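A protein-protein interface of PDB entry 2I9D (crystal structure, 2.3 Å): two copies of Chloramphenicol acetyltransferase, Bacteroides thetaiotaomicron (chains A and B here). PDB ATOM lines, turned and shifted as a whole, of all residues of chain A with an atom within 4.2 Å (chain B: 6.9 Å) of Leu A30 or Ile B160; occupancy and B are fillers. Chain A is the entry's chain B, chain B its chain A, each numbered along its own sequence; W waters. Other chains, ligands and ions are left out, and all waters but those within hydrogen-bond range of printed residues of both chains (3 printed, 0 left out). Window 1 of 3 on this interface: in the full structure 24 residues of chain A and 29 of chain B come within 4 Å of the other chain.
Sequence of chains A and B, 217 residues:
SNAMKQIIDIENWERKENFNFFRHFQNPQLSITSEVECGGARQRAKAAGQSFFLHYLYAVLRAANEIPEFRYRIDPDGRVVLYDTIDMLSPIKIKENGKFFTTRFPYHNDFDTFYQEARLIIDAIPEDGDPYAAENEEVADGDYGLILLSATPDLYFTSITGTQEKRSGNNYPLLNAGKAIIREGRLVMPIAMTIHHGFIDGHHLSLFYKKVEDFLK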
ATOM      1  N   GLN A  29      21.047 -16.036 -30.500  1.00  0.00           N
ATOM      2  CA  GLN A  29      21.588 -14.960 -31.343  1.00  0.00           C
ATOM      3  C   GLN A  29      21.699 -13.609 -30.649  1.00  0.00           C
ATOM      4  O   GLN A  29      21.050 -13.327 -29.656  1.00  0.00           O
ATOM      5  CB  GLN A  29      20.791 -14.800 -32.647  1.00  0.00           C
ATOM      6  CG  GLN A  29      20.551 -16.094 -33.361  1.00  0.00           C
ATOM      7  CD  GLN A  29      19.900 -15.917 -34.720  1.00  0.00           C
ATOM      8  OE1 GLN A  29      20.393 -16.473 -35.705  1.00  0.00           O
ATOM      9  NE2 GLN A  29      18.829 -15.121 -34.799  1.00  0.00           N
ATOM     10  N   LEU A  30      22.561 -12.779 -31.200  1.00  0.00           N
ATOM     11  CA  LEU A  30      22.584 -11.391 -30.805  1.00  0.00           C
ATOM     12  C   LEU A  30      22.677 -10.495 -32.025  1.00  0.00           C
ATOM     13  O   LEU A  30      23.199 -10.903 -33.067  1.00  0.00           O
ATOM     14  CB  LEU A  30      23.667 -11.136 -29.742  1.00  0.00           C
ATOM     15  CG  LEU A  30      25.084 -10.685 -29.915  1.00  0.00           C
ATOM     16  CD1 LEU A  30      25.108  -9.224 -30.337  1.00  0.00           C
ATOM     17  CD2 LEU A  30      25.776 -10.763 -28.561  1.00  0.00           C
ATOM     18  N   SER A  31      22.081  -9.315 -31.910  1.00  0.00           N
ATOM     19  CA  SER A  31      22.140  -8.275 -32.934  1.00  0.00           C
ATOM     20  C   SER A  31      22.945  -7.107 -32.448  1.00  0.00           C
ATOM     21  O   SER A  31      22.883  -6.719 -31.269  1.00  0.00           O
ATOM     22  CB  SER A  31      20.746  -7.781 -33.319  1.00  0.00           C
ATOM     23  OG  SER A  31      20.115  -8.787 -34.077  1.00  0.00           O
ATOM     24  N   ILE A  32      23.731  -6.575 -33.369  1.00  0.00           N
ATOM     25  CA  ILE A  32      24.568  -5.456 -33.071  1.00  0.00           C
ATOM     26  C   ILE A  32      24.505  -4.505 -34.250  1.00  0.00           C
ATOM     27  O   ILE A  32      24.358  -4.942 -35.419  1.00  0.00           O
ATOM     28  CB  ILE A  32      26.049  -5.887 -32.723  1.00  0.00           C
ATOM     29  CG1 ILE A  32      26.883  -4.664 -32.279  1.00  0.00           C
ATOM     30  CG2 ILE A  32      26.687  -6.684 -33.878  1.00  0.00           C
ATOM     31  CD1 ILE A  32      28.294  -5.004 -31.742  1.00  0.00           C
ATOM     32  N   MET A 193      24.128  -6.405 -37.675  1.00  0.00           N
ATOM     33  CA  MET A 193      24.268  -7.837 -37.925  1.00  0.00           C
ATOM     34  C   MET A 193      23.729  -8.721 -36.815  1.00  0.00           C
ATOM     35  O   MET A 193      23.751  -8.360 -35.654  1.00  0.00           O
ATOM     36  CB  MET A 193      25.726  -8.201 -38.233  1.00  0.00           C
ATOM     37  CG  MET A 193      26.643  -8.296 -37.018  1.00  0.00           C
ATOM     38  SD  MET A 193      28.584  -8.441 -37.531  1.00  0.00           S
ATOM     39  CE  MET A 193      28.464  -9.819 -38.870  1.00  0.00           C
ATOM     40  N   THR A 194      23.269  -9.900 -37.216  1.00  0.00           N
ATOM     41  CA  THR A 194      22.757 -10.901 -36.313  1.00  0.00           C
ATOM     42  C   THR A 194      23.663 -12.140 -36.354  1.00  0.00           C
ATOM     43  O   THR A 194      23.958 -12.660 -37.425  1.00  0.00           O
ATOM     44  CB  THR A 194      21.295 -11.184 -36.637  1.00  0.00           C
ATOM     45  OG1 THR A 194      20.545  -9.970 -36.392  1.00  0.00           O
ATOM     46  CG2 THR A 194      20.727 -12.362 -35.768  1.00  0.00           C
ATOM     47  N   ILE A 195      24.153 -12.573 -35.191  1.00  0.00           N
ATOM     48  CA  ILE A 195      25.105 -13.690 -35.127  1.00  0.00           C
ATOM     49  C   ILE A 195      24.718 -14.689 -34.035  1.00  0.00           C
ATOM     50  O   ILE A 195      23.874 -14.382 -33.204  1.00  0.00           O
ATOM     51  CB  ILE A 195      26.618 -13.197 -34.995  1.00  0.00           C
ATOM     52  CG1 ILE A 195      26.859 -12.210 -33.835  1.00  0.00           C
ATOM     53  CG2 ILE A 195      27.084 -12.555 -36.291  1.00  0.00           C
ATOM     54  CD1 ILE A 195      26.763 -12.814 -32.356  1.00  0.00           C
ATOM     55  N   HIS A 197      25.789 -16.405 -30.655  1.00  0.00           N
ATOM     56  CA  HIS A 197      26.682 -16.106 -29.563  1.00  0.00           C
ATOM     57  C   HIS A 197      27.593 -17.308 -29.207  1.00  0.00           C
ATOM     58  O   HIS A 197      28.677 -17.127 -28.642  1.00  0.00           O
ATOM     59  CB  HIS A 197      25.886 -15.580 -28.348  1.00  0.00           C
ATOM     60  CG  HIS A 197      26.704 -14.743 -27.411  1.00  0.00           C
ATOM     61  ND1 HIS A 197      28.085 -14.844 -27.327  1.00  0.00           N
ATOM     62  CD2 HIS A 197      26.337 -13.803 -26.503  1.00  0.00           C
ATOM     63  CE1 HIS A 197      28.534 -13.987 -26.420  1.00  0.00           C
ATOM     64  NE2 HIS A 197      27.497 -13.339 -25.911  1.00  0.00           N
ATOM     65  N   LEU A 205      33.357  -9.233 -32.443  1.00  0.00           N
ATOM     66  CA  LEU A 205      32.555  -8.160 -33.056  1.00  0.00           C
ATOM     67  C   LEU A 205      33.374  -6.887 -33.165  1.00  0.00           C
ATOM     68  O   LEU A 205      33.342  -6.191 -34.173  1.00  0.00           O
ATOM     69  CB  LEU A 205      31.268  -7.927 -32.240  1.00  0.00           C
ATOM     70  CG  LEU A 205      30.262  -9.093 -32.277  1.00  0.00           C
ATOM     71  CD1 LEU A 205      29.171  -9.004 -31.169  1.00  0.00           C
ATOM     72  CD2 LEU A 205      29.641  -9.318 -33.663  1.00  0.00           C
ATOM     73  N   SER B  31      15.221  -5.060 -25.188  1.00  0.00           N
ATOM     74  CA  SER B  31      16.594  -4.518 -25.174  1.00  0.00           C
ATOM     75  C   SER B  31      16.594  -3.038 -25.492  1.00  0.00           C
ATOM     76  O   SER B  31      15.815  -2.558 -26.306  1.00  0.00           O
ATOM     77  CB  SER B  31      17.517  -5.237 -26.172  1.00  0.00           C
ATOM     78  OG  SER B  31      17.462  -6.627 -26.003  1.00  0.00           O
ATOM     79  N   ILE B  32      17.519  -2.318 -24.887  1.00  0.00           N
ATOM     80  CA  ILE B  32      17.628  -0.902 -25.165  1.00  0.00           C
ATOM     81  C   ILE B  32      19.099  -0.568 -25.125  1.00  0.00           C
ATOM     82  O   ILE B  32      19.836  -1.168 -24.343  1.00  0.00           O
ATOM     83  CB  ILE B  32      16.831  -0.045 -24.115  1.00  0.00           C
ATOM     84  CG1 ILE B  32      17.003   1.468 -24.364  1.00  0.00           C
ATOM     85  CG2 ILE B  32      17.208  -0.453 -22.652  1.00  0.00           C
ATOM     86  CD1 ILE B  32      16.023   2.339 -23.573  1.00  0.00           C
ATOM     87  N   THR B  33      19.522   0.354 -25.988  1.00  0.00           N
ATOM     88  CA  THR B  33      20.844   0.977 -25.898  1.00  0.00           C
ATOM     89  C   THR B  33      20.707   2.499 -25.771  1.00  0.00           C
ATOM     90  O   THR B  33      19.905   3.122 -26.484  1.00  0.00           O
ATOM     91  CB  THR B  33      21.708   0.641 -27.121  1.00  0.00           C
ATOM     92  OG1 THR B  33      21.679  -0.771 -27.320  1.00  0.00           O
ATOM     93  CG2 THR B  33      23.151   1.116 -26.925  1.00  0.00           C
ATOM     94  N   SER B 150      29.008  -7.049 -19.776  1.00  0.00           N
ATOM     95  CA  SER B 150      30.113  -7.432 -20.637  1.00  0.00           C
ATOM     96  C   SER B 150      30.711  -6.169 -21.300  1.00  0.00           C
ATOM     97  O   SER B 150      29.983  -5.413 -21.924  1.00  0.00           O
ATOM     98  CB  SER B 150      29.608  -8.448 -21.665  1.00  0.00           C
ATOM     99  OG  SER B 150      30.566  -8.584 -22.687  1.00  0.00           O
ATOM    100  N   THR B 152      33.077  -4.059 -23.995  1.00  0.00           N
ATOM    101  CA  THR B 152      33.826  -4.085 -25.226  1.00  0.00           C
ATOM    102  C   THR B 152      34.421  -2.710 -25.394  1.00  0.00           C
ATOM    103  O   THR B 152      33.861  -1.877 -26.134  1.00  0.00           O
ATOM    104  CB  THR B 152      32.999  -4.562 -26.500  1.00  0.00           C
ATOM    105  OG1 THR B 152      31.999  -3.603 -26.823  1.00  0.00           O
ATOM    106  CG2 THR B 152      32.318  -5.821 -26.208  1.00  0.00           C
ATOM    107  N   LEU B 155      35.027  -0.959 -28.872  1.00  0.00           N
ATOM    108  CA  LEU B 155      33.916  -0.893 -29.800  1.00  0.00           C
ATOM    109  C   LEU B 155      32.835   0.086 -29.341  1.00  0.00           C
ATOM    110  O   LEU B 155      32.299  -0.045 -28.236  1.00  0.00           O
ATOM    111  CB  LEU B 155      33.295  -2.288 -29.960  1.00  0.00           C
ATOM    112  CG  LEU B 155      32.095  -2.453 -30.914  1.00  0.00           C
ATOM    113  CD1 LEU B 155      32.396  -1.878 -32.302  1.00  0.00           C
ATOM    114  CD2 LEU B 155      31.642  -3.920 -31.007  1.00  0.00           C
ATOM    115  N   PHE B 157      29.088   1.015 -30.148  1.00  0.00           N
ATOM    116  CA  PHE B 157      27.941   0.375 -30.827  1.00  0.00           C
ATOM    117  C   PHE B 157      26.702   1.229 -30.557  1.00  0.00           C
ATOM    118  O   PHE B 157      26.652   1.946 -29.549  1.00  0.00           O
ATOM    119  CB  PHE B 157      27.734  -1.057 -30.319  1.00  0.00           C
ATOM    120  CG  PHE B 157      27.665  -1.176 -28.795  1.00  0.00           C
ATOM    121  CD1 PHE B 157      26.475  -0.878 -28.107  1.00  0.00           C
ATOM    122  CD2 PHE B 157      28.785  -1.611 -28.047  1.00  0.00           C
ATOM    123  CE1 PHE B 157      26.398  -0.987 -26.700  1.00  0.00           C
ATOM    124  CE2 PHE B 157      28.714  -1.726 -26.631  1.00  0.00           C
ATOM    125  CZ  PHE B 157      27.509  -1.416 -25.963  1.00  0.00           C
ATOM    126  N   THR B 158      25.710   1.151 -31.442  1.00  0.00           N
ATOM    127  CA  THR B 158      24.458   1.852 -31.200  1.00  0.00           C
ATOM    128  C   THR B 158      23.357   0.901 -30.750  1.00  0.00           C
ATOM    129  O   THR B 158      22.286   1.350 -30.309  1.00  0.00           O
ATOM    130  CB  THR B 158      23.958   2.619 -32.443  1.00  0.00           C
ATOM    131  OG1 THR B 158      24.074   1.781 -33.593  1.00  0.00           O
ATOM    132  CG2 THR B 158      24.757   3.881 -32.651  1.00  0.00           C
ATOM    133  N   SER B 159      23.621  -0.404 -30.857  1.00  0.00           N
ATOM    134  CA  SER B 159      22.680  -1.422 -30.480  1.00  0.00           C
ATOM    135  C   SER B 159      23.388  -2.748 -30.171  1.00  0.00           C
ATOM    136  O   SER B 159      24.237  -3.199 -30.940  1.00  0.00           O
ATOM    137  CB  SER B 159      21.691  -1.604 -31.631  1.00  0.00           C
ATOM    138  OG  SER B 159      20.819  -2.705 -31.413  1.00  0.00           O
ATOM    139  N   ILE B 160      23.048  -3.355 -29.033  1.00  0.00           N
ATOM    140  CA  ILE B 160      23.288  -4.780 -28.792  1.00  0.00           C
ATOM    141  C   ILE B 160      22.001  -5.340 -28.178  1.00  0.00           C
ATOM    142  O   ILE B 160      21.504  -4.815 -27.193  1.00  0.00           O
ATOM    143  CB  ILE B 160      24.514  -5.080 -27.876  1.00  0.00           C
ATOM    144  CG1 ILE B 160      25.819  -4.686 -28.568  1.00  0.00           C
ATOM    145  CG2 ILE B 160      24.556  -6.592 -27.520  1.00  0.00           C
ATOM    146  CD1 ILE B 160      27.094  -4.745 -27.734  1.00  0.00           C
ATOM    147  N   THR B 161      21.446  -6.384 -28.780  1.00  0.00           N
ATOM    148  CA  THR B 161      20.317  -7.075 -28.175  1.00  0.00           C
ATOM    149  C   THR B 161      20.802  -8.309 -27.414  1.00  0.00           C
ATOM    150  O   THR B 161      21.815  -8.929 -27.780  1.00  0.00           O
ATOM    151  CB  THR B 161      19.356  -7.566 -29.227  1.00  0.00           C
ATOM    152  OG1 THR B 161      20.028  -8.603 -29.957  1.00  0.00           O
ATOM    153  CG2 THR B 161      18.928  -6.425 -30.132  1.00  0.00           C
ATOM    154  N   GLY B 162      20.091  -8.686 -26.365  1.00  0.00           N
ATOM    155  CA  GLY B 162      20.449  -9.872 -25.634  1.00  0.00           C
ATOM    156  C   GLY B 162      19.910 -11.153 -26.246  1.00  0.00           C
ATOM    157  O   GLY B 162      18.913 -11.157 -27.018  1.00  0.00           O
ATOM    158  N   THR B 163      20.596 -12.246 -25.900  1.00  0.00           N
ATOM    159  CA  THR B 163      20.082 -13.601 -26.070  1.00  0.00           C
ATOM    160  C   THR B 163      18.856 -13.841 -25.163  1.00  0.00           C
ATOM    161  O   THR B 163      18.528 -13.031 -24.300  1.00  0.00           O
ATOM    162  CB  THR B 163      21.195 -14.651 -25.765  1.00  0.00           C
ATOM    163  OG1 THR B 163      21.839 -14.313 -24.543  1.00  0.00           O
ATOM    164  CG2 THR B 163      22.229 -14.661 -26.854  1.00  0.00           C
ATOM    165  N   LEU B 175      23.813  -6.840 -19.671  1.00  0.00           N
ATOM    166  CA  LEU B 175      24.226  -5.502 -20.100  1.00  0.00           C
ATOM    167  C   LEU B 175      25.523  -5.590 -20.886  1.00  0.00           C
ATOM    168  O   LEU B 175      26.276  -6.571 -20.764  1.00  0.00           O
ATOM    169  CB  LEU B 175      24.426  -4.529 -18.918  1.00  0.00           C
ATOM    170  CG  LEU B 175      23.197  -4.103 -18.105  1.00  0.00           C
ATOM    171  CD1 LEU B 175      22.960  -5.025 -16.884  1.00  0.00           C
ATOM    172  CD2 LEU B 175      23.339  -2.665 -17.671  1.00  0.00           C
ATOM    173  N   ASN B 176      25.749  -4.560 -21.691  1.00  0.00           N
ATOM    174  CA  ASN B 176      26.936  -4.384 -22.485  1.00  0.00           C
ATOM    175  C   ASN B 176      27.373  -2.949 -22.393  1.00  0.00           C
ATOM    176  O   ASN B 176      26.533  -2.035 -22.521  1.00  0.00           O
ATOM    177  CB  ASN B 176      26.622  -4.658 -23.940  1.00  0.00           C
ATOM    178  CG  ASN B 176      26.239  -6.096 -24.184  1.00  0.00           C
ATOM    179  OD1 ASN B 176      27.105  -6.953 -24.368  1.00  0.00           O
ATOM    180  ND2 ASN B 176      24.939  -6.366 -24.219  1.00  0.00           N
ATOM    181  N   ALA B 177      28.675  -2.749 -22.206  1.00  0.00           N
ATOM    182  CA  ALA B 177      29.271  -1.423 -22.183  1.00  0.00           C
ATOM    183  C   ALA B 177      30.188  -1.353 -23.401  1.00  0.00           C
ATOM    184  O   ALA B 177      30.800  -2.360 -23.781  1.00  0.00           O
ATOM    185  CB  ALA B 177      30.040  -1.221 -20.904  1.00  0.00           C
ATOM    186  N   GLY B 178      30.256  -0.196 -24.034  1.00  0.00           N
ATOM    187  CA  GLY B 178      31.112  -0.035 -25.200  1.00  0.00           C
ATOM    188  C   GLY B 178      32.153   1.024 -24.993  1.00  0.00           C
ATOM    189  O   GLY B 178      32.322   1.526 -23.882  1.00  0.00           O
ATOM    190  N   ALA B 192      24.010  -0.964 -23.353  1.00  0.00           N
ATOM    191  CA  ALA B 192      22.880  -1.739 -23.802  1.00  0.00           C
ATOM    192  C   ALA B 192      22.411  -2.606 -22.627  1.00  0.00           C
ATOM    193  O   ALA B 192      23.207  -2.947 -21.729  1.00  0.00           O
ATOM    194  CB  ALA B 192      23.292  -2.610 -24.977  1.00  0.00           C
ATOM    195  N   MET B 193      21.125  -2.950 -22.623  1.00  0.00           N
ATOM    196  CA  MET B 193      20.611  -3.869 -21.635  1.00  0.00           C
ATOM    197  C   MET B 193      19.351  -4.595 -22.090  1.00  0.00           C
ATOM    198  O   MET B 193      18.591  -4.097 -22.904  1.00  0.00           O
ATOM    199  CB  MET B 193      20.398  -3.167 -20.284  1.00  0.00           C
ATOM    200  CG  MET B 193      19.320  -2.103 -20.279  1.00  0.00           C
ATOM    201  SD  MET B 193      19.215  -1.068 -18.572  1.00  0.00           S
ATOM    202  CE  MET B 193      19.491  -2.547 -17.260  1.00  0.00           C
ATOM    203  N   THR B 194      19.162  -5.791 -21.535  1.00  0.00           N
ATOM    204  CA  THR B 194      18.010  -6.630 -21.796  1.00  0.00           C
ATOM    205  C   THR B 194      17.301  -6.946 -20.476  1.00  0.00           C
ATOM    206  O   THR B 194      17.890  -7.491 -19.553  1.00  0.00           O
ATOM    207  CB  THR B 194      18.435  -7.889 -22.561  1.00  0.00           C
ATOM    208  OG1 THR B 194      18.929  -7.470 -23.820  1.00  0.00           O
ATOM    209  CG2 THR B 194      17.270  -8.875 -22.797  1.00  0.00           C
HETATM  210  O   HOH W   1      18.965 -11.269 -29.822  1.00  0.00           O
HETATM  211  O   HOH W   2      21.450  -4.129 -33.878  1.00  0.00           O
HETATM  212  O   HOH W   3      18.792 -10.827 -32.261  1.00  0.00           O
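N of Ile B160 lies within hydrogen-bond range of OG1 of Thr B33 (3.4 Å). N of Ile A195 is in hydrogen-bond range of O of Leu A30, 2.9 Å away. The side-chain hydroxyl (OG) of Ser A31 is in hydrogen-bond range of the side-chain hydroxyl (OG1) of Thr A194, 2.6 Å away. The backbone carbonyl oxygen (O) of Ile A32 sits at hydrogen-bond distance from the backbone NH (N) of Met A193 (2.7 Å).
The backbone carbonyl oxygen of Ser A31 is in hydrogen-bond range of the backbone NH of Thr B161, at 2.9 Å.
4 positions are printed for both chains. Of the 9 pairs that touch across the chains among the printed residues, none has its exchanged pair printed and touching as well.
Water W1 lies within hydrogen-bond range of the backbone carbonyl oxygen of Gly B162, the side-chain hydroxyl of Thr B161 and the backbone carbonyl oxygen of Gln A29. Water W2 lies within hydrogen-bond range of the side-chain hydroxyl (OG) of Ser B159 and the backbone NH (N) of Ile A32. Water W3 lies within hydrogen-bond range of the side-chain hydroxyl of Ser A31 and the side-chain hydroxyl of Thr B161.
Printed residues of chain A that touch a printed residue of chain B: Gln A29, Leu A30, Ser A31 and Ile A32. Hydrophobic or aromatic side chains of chain A within 4 Å of the printed part of chain B: Leu A30 and Ile A32. Along chain A the printed residues that touch a printed residue of chain B span positions 29 to 32. Hydrophobic or aromatic side chains of chain B that line the printed part of chain A: Leu B155 and Ile B160. Among the printed residues, 9 pairs touch across the chains.
Among the printed residues, merely in contact across the chains: Ile A32 with Ser B159, Ser A31 with Ile B160, Gln A29 with Thr B163, Leu A30 with Thr B161, Ile A32 with Leu B155, Ser A31 with Ser B159, Ile A32 with Ile B160 and Leu A30 with Ile B160.
Leu A30 touches just these residues of chain B: Ile B160 and Thr B161. Leu A205 touches none of the printed residues of chain B. Of the printed residues of chain A, Ser B159 touches Ser A31 (3.8 Å) and Ile A32 (3.1 Å). Printed residues of chain A within 4 Å of Ile B160: Leu A30, Ser A31 and Ile A32. Of the printed residues of chain A, Thr B161 touches Leu A30 (3.5 Å) and Ser A31 (2.9 Å). Printed residues of chain A within 4 Å of Thr B163: Gln A29. The nearest printed residue of chain A that does not touch Ile B160 is Leu A205 (5.9 Å).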
